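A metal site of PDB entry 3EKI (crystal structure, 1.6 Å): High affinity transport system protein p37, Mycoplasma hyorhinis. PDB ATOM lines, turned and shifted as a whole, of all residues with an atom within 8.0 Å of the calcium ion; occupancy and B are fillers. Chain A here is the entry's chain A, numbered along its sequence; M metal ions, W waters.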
ATOM      1  N   TRP A  42      23.491  28.943  10.428  1.00  0.00           N
ATOM      2  CA  TRP A  42      22.294  29.491  11.078  1.00  0.00           C
ATOM      3  C   TRP A  42      21.351  29.985  10.011  1.00  0.00           C
ATOM      4  O   TRP A  42      21.705  30.711   9.077  1.00  0.00           O
ATOM      5  CB  TRP A  42      22.656  30.638  12.022  1.00  0.00           C
ATOM      6  CG  TRP A  42      21.495  31.097  12.861  1.00  0.00           C
ATOM      7  CD1 TRP A  42      20.605  32.079  12.583  1.00  0.00           C
ATOM      8  CD2 TRP A  42      21.151  30.525  14.139  1.00  0.00           C
ATOM      9  NE1 TRP A  42      19.709  32.185  13.613  1.00  0.00           N
ATOM     10  CE2 TRP A  42      20.022  31.247  14.584  1.00  0.00           C
ATOM     11  CE3 TRP A  42      21.691  29.505  14.945  1.00  0.00           C
ATOM     12  CZ2 TRP A  42      19.422  30.938  15.804  1.00  0.00           C
ATOM     13  CZ3 TRP A  42      21.082  29.227  16.153  1.00  0.00           C
ATOM     14  CH2 TRP A  42      19.953  29.935  16.595  1.00  0.00           C
ATOM     15  N   ASP A  43      20.075  29.616  10.086  1.00  0.00           N
ATOM     16  CA  ASP A  43      19.126  30.021   9.072  1.00  0.00           C
ATOM     17  C   ASP A  43      18.055  30.866   9.730  1.00  0.00           C
ATOM     18  O   ASP A  43      17.380  30.343  10.634  1.00  0.00           O
ATOM     19  CB  ASP A  43      18.524  28.780   8.411  1.00  0.00           C
ATOM     20  CG  ASP A  43      17.690  29.071   7.206  1.00  0.00           C
ATOM     21  OD1 ASP A  43      17.464  30.276   6.903  1.00  0.00           O
ATOM     22  OD2 ASP A  43      17.247  28.123   6.518  1.00  0.00           O
ATOM     23  N   LYS A  44      17.902  32.120   9.353  1.00  0.00           N
ATOM     24  CA  LYS A  44      16.955  33.001  10.033  1.00  0.00           C
ATOM     25  C   LYS A  44      15.523  32.772   9.627  1.00  0.00           C
ATOM     26  O   LYS A  44      14.598  33.413  10.165  1.00  0.00           O
ATOM     27  CB  LYS A  44      17.341  34.469   9.785  1.00  0.00           C
ATOM     28  CG  LYS A  44      17.142  34.859   8.319  1.00  0.00           C
ATOM     29  CD  LYS A  44      17.749  36.223   7.992  1.00  0.00           C
ATOM     30  CE  LYS A  44      17.448  36.606   6.554  1.00  0.00           C
ATOM     31  NZ  LYS A  44      18.574  37.371   5.947  1.00  0.00           N
ATOM     32  N   SER A  45      15.270  31.850   8.719  1.00  0.00           N
ATOM     33  CA  SER A  45      13.938  31.487   8.265  1.00  0.00           C
ATOM     34  C   SER A  45      13.840  29.962   8.319  1.00  0.00           C
ATOM     35  O   SER A  45      14.617  29.275   7.646  1.00  0.00           O
ATOM     36  CB  SER A  45      13.674  31.984   6.851  1.00  0.00           C
ATOM     37  OG  SER A  45      12.484  31.435   6.293  1.00  0.00           O
ATOM     38  N   ILE A  46      12.928  29.416   9.125  1.00  0.00           N
ATOM     39  CA  ILE A  46      12.774  27.972   9.181  1.00  0.00           C
ATOM     40  C   ILE A  46      11.389  27.636   8.633  1.00  0.00           C
ATOM     41  O   ILE A  46      10.424  28.222   9.102  1.00  0.00           O
ATOM     42  CB  ILE A  46      13.010  27.485  10.606  1.00  0.00           C
ATOM     43  CG1 ILE A  46      14.463  27.595  11.083  1.00  0.00           C
ATOM     44  CG2 ILE A  46      12.508  26.047  10.796  1.00  0.00           C
ATOM     45  CD1 ILE A  46      15.364  26.542  10.459  1.00  0.00           C
ATOM     46  N   THR A  47      11.360  26.751   7.665  1.00  0.00           N
ATOM     47  CA  THR A  47      10.128  26.289   7.050  1.00  0.00           C
ATOM     48  C   THR A  47       9.909  24.799   7.329  1.00  0.00           C
ATOM     49  O   THR A  47      10.765  23.992   6.954  1.00  0.00           O
ATOM     50  CB  THR A  47      10.166  26.528   5.525  1.00  0.00           C
ATOM     51  OG1 THR A  47      10.298  27.934   5.267  1.00  0.00           O
ATOM     52  CG2 THR A  47       8.870  26.072   4.881  1.00  0.00           C
ATOM     53  N   PHE A  48       8.806  24.450   7.957  1.00  0.00           N
ATOM     54  CA  PHE A  48       8.361  23.085   8.168  1.00  0.00           C
ATOM     55  C   PHE A  48       7.483  22.582   7.022  1.00  0.00           C
ATOM     56  O   PHE A  48       6.541  23.251   6.576  1.00  0.00           O
ATOM     57  CB  PHE A  48       7.570  22.998   9.475  1.00  0.00           C
ATOM     58  CG  PHE A  48       8.323  23.374  10.747  1.00  0.00           C
ATOM     59  CD1 PHE A  48       9.699  23.287  10.845  1.00  0.00           C
ATOM     60  CD2 PHE A  48       7.608  23.807  11.844  1.00  0.00           C
ATOM     61  CE1 PHE A  48      10.329  23.645  12.043  1.00  0.00           C
ATOM     62  CE2 PHE A  48       8.222  24.151  13.035  1.00  0.00           C
ATOM     63  CZ  PHE A  48       9.593  24.042  13.131  1.00  0.00           C
ATOM     64  N   VAL A  96      14.717  34.113  14.466  1.00  0.00           N
ATOM     65  CA  VAL A  96      14.204  33.211  13.454  1.00  0.00           C
ATOM     66  C   VAL A  96      12.699  33.323  13.280  1.00  0.00           C
ATOM     67  O   VAL A  96      11.959  33.393  14.266  1.00  0.00           O
ATOM     68  CB  VAL A  96      14.568  31.762  13.851  1.00  0.00           C
ATOM     69  CG1 VAL A  96      14.087  30.791  12.795  1.00  0.00           C
ATOM     70  CG2 VAL A  96      16.083  31.667  14.014  1.00  0.00           C
ATOM     71  N   ASP A  97      12.288  33.347  12.024  1.00  0.00           N
ATOM     72  CA  ASP A  97      10.886  33.272  11.619  1.00  0.00           C
ATOM     73  C   ASP A  97      10.516  31.832  11.249  1.00  0.00           C
ATOM     74  O   ASP A  97      11.347  31.107  10.691  1.00  0.00           O
ATOM     75  CB  ASP A  97      10.597  34.130  10.390  1.00  0.00           C
ATOM     76  CG  ASP A  97       9.124  34.155  10.038  1.00  0.00           C
ATOM     77  OD1 ASP A  97       8.325  34.202  11.000  1.00  0.00           O
ATOM     78  OD2 ASP A  97       8.770  34.107   8.847  1.00  0.00           O
ATOM     79  N   LYS A  99       7.731  29.190   9.285  1.00  0.00           N
ATOM     80  CA  LYS A  99       6.758  29.112   8.218  1.00  0.00           C
ATOM     81  C   LYS A  99       6.433  27.630   7.976  1.00  0.00           C
ATOM     82  O   LYS A  99       7.165  26.802   8.489  1.00  0.00           O
ATOM     83  CB  LYS A  99       7.252  29.756   6.927  1.00  0.00           C
ATOM     84  CG  LYS A  99       7.717  31.194   7.076  1.00  0.00           C
ATOM     85  CD  LYS A  99       8.074  31.756   5.705  1.00  0.00           C
ATOM     86  CE  LYS A  99       9.481  32.336   5.677  1.00  0.00           C
ATOM     87  NZ  LYS A  99       9.948  32.530   4.273  1.00  0.00           N
ATOM     88  N   ASN A 117      18.116  22.405   0.599  1.00  0.00           N
ATOM     89  CA  ASN A 117      17.714  23.705   0.096  1.00  0.00           C
ATOM     90  C   ASN A 117      17.053  24.458   1.243  1.00  0.00           C
ATOM     91  O   ASN A 117      16.121  23.899   1.839  1.00  0.00           O
ATOM     92  CB  ASN A 117      16.763  23.557  -1.087  1.00  0.00           C
ATOM     93  CG  ASN A 117      16.348  24.829  -1.762  1.00  0.00           C
ATOM     94  OD1 ASN A 117      15.869  25.784  -1.163  1.00  0.00           O
ATOM     95  ND2 ASN A 117      16.522  24.891  -3.085  1.00  0.00           N
ATOM     96  N   PRO A 118      17.478  25.663   1.588  1.00  0.00           N
ATOM     97  CA  PRO A 118      16.867  26.374   2.709  1.00  0.00           C
ATOM     98  C   PRO A 118      15.395  26.696   2.586  1.00  0.00           C
ATOM     99  O   PRO A 118      14.775  27.177   3.546  1.00  0.00           O
ATOM    100  CB  PRO A 118      17.666  27.687   2.787  1.00  0.00           C
ATOM    101  CG  PRO A 118      18.946  27.384   2.088  1.00  0.00           C
ATOM    102  CD  PRO A 118      18.613  26.397   0.995  1.00  0.00           C
ATOM    103  N   GLU A 119      14.725  26.467   1.456  1.00  0.00           N
ATOM    104  CA  GLU A 119      13.299  26.666   1.350  1.00  0.00           C
ATOM    105  C   GLU A 119      12.511  25.604   2.118  1.00  0.00           C
ATOM    106  O   GLU A 119      11.326  25.835   2.379  1.00  0.00           O
ATOM    107  CB  GLU A 119      12.806  26.662  -0.105  1.00  0.00           C
ATOM    108  CG  GLU A 119      12.447  25.311  -0.682  1.00  0.00           C
ATOM    109  CD  GLU A 119      12.725  25.232  -2.174  1.00  0.00           C
ATOM    110  OE1 GLU A 119      12.531  26.258  -2.863  1.00  0.00           O
ATOM    111  OE2 GLU A 119      13.142  24.143  -2.619  1.00  0.00           O
ATOM    112  N   LEU A 120      13.147  24.499   2.485  1.00  0.00           N
ATOM    113  CA  LEU A 120      12.501  23.444   3.274  1.00  0.00           C
ATOM    114  C   LEU A 120      13.520  22.865   4.245  1.00  0.00           C
ATOM    115  O   LEU A 120      14.485  22.204   3.873  1.00  0.00           O
ATOM    116  CB  LEU A 120      11.917  22.324   2.397  1.00  0.00           C
ATOM    117  CG  LEU A 120      11.350  21.133   3.179  1.00  0.00           C
ATOM    118  CD1 LEU A 120      10.133  21.565   3.981  1.00  0.00           C
ATOM    119  CD2 LEU A 120      11.029  20.015   2.213  1.00  0.00           C
ATOM    120  N   ASP A 121      13.304  23.146   5.528  1.00  0.00           N
ATOM    121  CA  ASP A 121      14.300  22.859   6.552  1.00  0.00           C
ATOM    122  C   ASP A 121      14.007  21.636   7.430  1.00  0.00           C
ATOM    123  O   ASP A 121      14.939  21.053   7.990  1.00  0.00           O
ATOM    124  CB  ASP A 121      14.427  24.090   7.448  1.00  0.00           C
ATOM    125  CG  ASP A 121      14.720  25.365   6.676  1.00  0.00           C
ATOM    126  OD1 ASP A 121      13.850  26.254   6.561  1.00  0.00           O
ATOM    127  OD2 ASP A 121      15.826  25.439   6.091  1.00  0.00           O
ATOM    128  N   PHE A 122      12.732  21.288   7.584  1.00  0.00           N
ATOM    129  CA  PHE A 122      12.395  20.249   8.539  1.00  0.00           C
ATOM    130  C   PHE A 122      11.039  19.654   8.200  1.00  0.00           C
ATOM    131  O   PHE A 122      10.162  20.297   7.649  1.00  0.00           O
ATOM    132  CB  PHE A 122      12.358  20.840   9.941  1.00  0.00           C
ATOM    133  CG  PHE A 122      11.880  20.026  11.104  1.00  0.00           C
ATOM    134  CD1 PHE A 122      12.776  19.297  11.861  1.00  0.00           C
ATOM    135  CD2 PHE A 122      10.529  20.015  11.435  1.00  0.00           C
ATOM    136  CE1 PHE A 122      12.328  18.550  12.946  1.00  0.00           C
ATOM    137  CE2 PHE A 122      10.061  19.269  12.506  1.00  0.00           C
ATOM    138  CZ  PHE A 122      10.998  18.568  13.242  1.00  0.00           C
ATOM    139  N   ARG A 349      17.059  18.987   7.135  1.00  0.00           N
ATOM    140  CA  ARG A 349      18.098  19.064   6.111  1.00  0.00           C
ATOM    141  C   ARG A 349      19.445  19.227   6.842  1.00  0.00           C
ATOM    142  O   ARG A 349      19.557  19.763   7.940  1.00  0.00           O
ATOM    143  CB  ARG A 349      17.840  20.128   5.073  1.00  0.00           C
ATOM    144  CG  ARG A 349      17.872  21.546   5.612  1.00  0.00           C
ATOM    145  CD  ARG A 349      17.724  22.624   4.546  1.00  0.00           C
ATOM    146  NE  ARG A 349      17.877  23.956   5.134  1.00  0.00           N
ATOM    147  CZ  ARG A 349      18.964  24.659   5.322  1.00  0.00           C
ATOM    148  NH1 ARG A 349      20.138  24.180   4.951  1.00  0.00           N
ATOM    149  NH2 ARG A 349      18.900  25.862   5.887  1.00  0.00           N
ATOM    150  N   VAL A 352      21.281  22.678   8.416  1.00  0.00           N
ATOM    151  CA  VAL A 352      20.792  23.564   9.463  1.00  0.00           C
ATOM    152  C   VAL A 352      21.733  23.518  10.643  1.00  0.00           C
ATOM    153  O   VAL A 352      22.131  22.433  11.115  1.00  0.00           O
ATOM    154  CB  VAL A 352      19.370  23.173   9.948  1.00  0.00           C
ATOM    155  CG1 VAL A 352      19.037  23.980  11.183  1.00  0.00           C
ATOM    156  CG2 VAL A 352      18.379  23.356   8.830  1.00  0.00           C
ATOM    157  N   GLU A 356      20.824  25.475  16.329  1.00  0.00           N
ATOM    158  CA  GLU A 356      19.447  25.785  15.919  1.00  0.00           C
ATOM    159  C   GLU A 356      18.574  24.532  15.954  1.00  0.00           C
ATOM    160  O   GLU A 356      17.428  24.599  16.424  1.00  0.00           O
ATOM    161  CB  GLU A 356      19.461  26.442  14.542  1.00  0.00           C
ATOM    162  CG  GLU A 356      18.136  27.096  14.165  1.00  0.00           C
ATOM    163  CD  GLU A 356      18.195  27.911  12.893  1.00  0.00           C
ATOM    164  OE1 GLU A 356      19.220  27.791  12.191  1.00  0.00           O
ATOM    165  OE2 GLU A 356      17.241  28.660  12.594  1.00  0.00           O
HETATM  166 CA    CA M   1      14.996  28.002   5.674  1.00  0.00          CA
HETATM  167  O   HOH W   1      12.675  29.128   5.231  1.00  0.00           O
HETATM  168  O   HOH W   2      15.652  30.195   4.578  1.00  0.00           O
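The calcium ion is bound by the side-chain carboxylate (OD1) of Asp 121 (2.3 Å), the backbone carbonyl oxygen (O) of Pro 118 (2.3 Å), the backbone carbonyl oxygen (O) of Ser 45 (2.4 Å), the side-chain carboxylate (OD2) of Asp 43 (2.4 Å), water W2 (2.5 Å), water W1 (2.6 Å) and the side-chain carboxylate (OD2) of Asp 121 (2.7 Å).
Water W1 bridges the side-chain hydroxyl (OG) of Ser 45 (2.5 Å) and the side-chain hydroxyl (OG1) of Thr 47 (2.7 Å).
Within 4 Å of the calcium ion: Asp 43, Ser 45, Pro 118 and Asp 121.
N of Asp 121 sits at hydrogen-bond distance from O of Thr 47 (3.0 Å). O of Asp 121 is in hydrogen-bond range of N of Arg 349 (3.1 Å). OG of Ser 45 lies close to NZ of Lys 99, 3.4 Å away. NH2 of Arg 349 sits close to OD2 of Asp 43 (2.9 Å). N of Asp 43 is in hydrogen-bond range of OE1 of Glu 356, at 2.9 Å.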
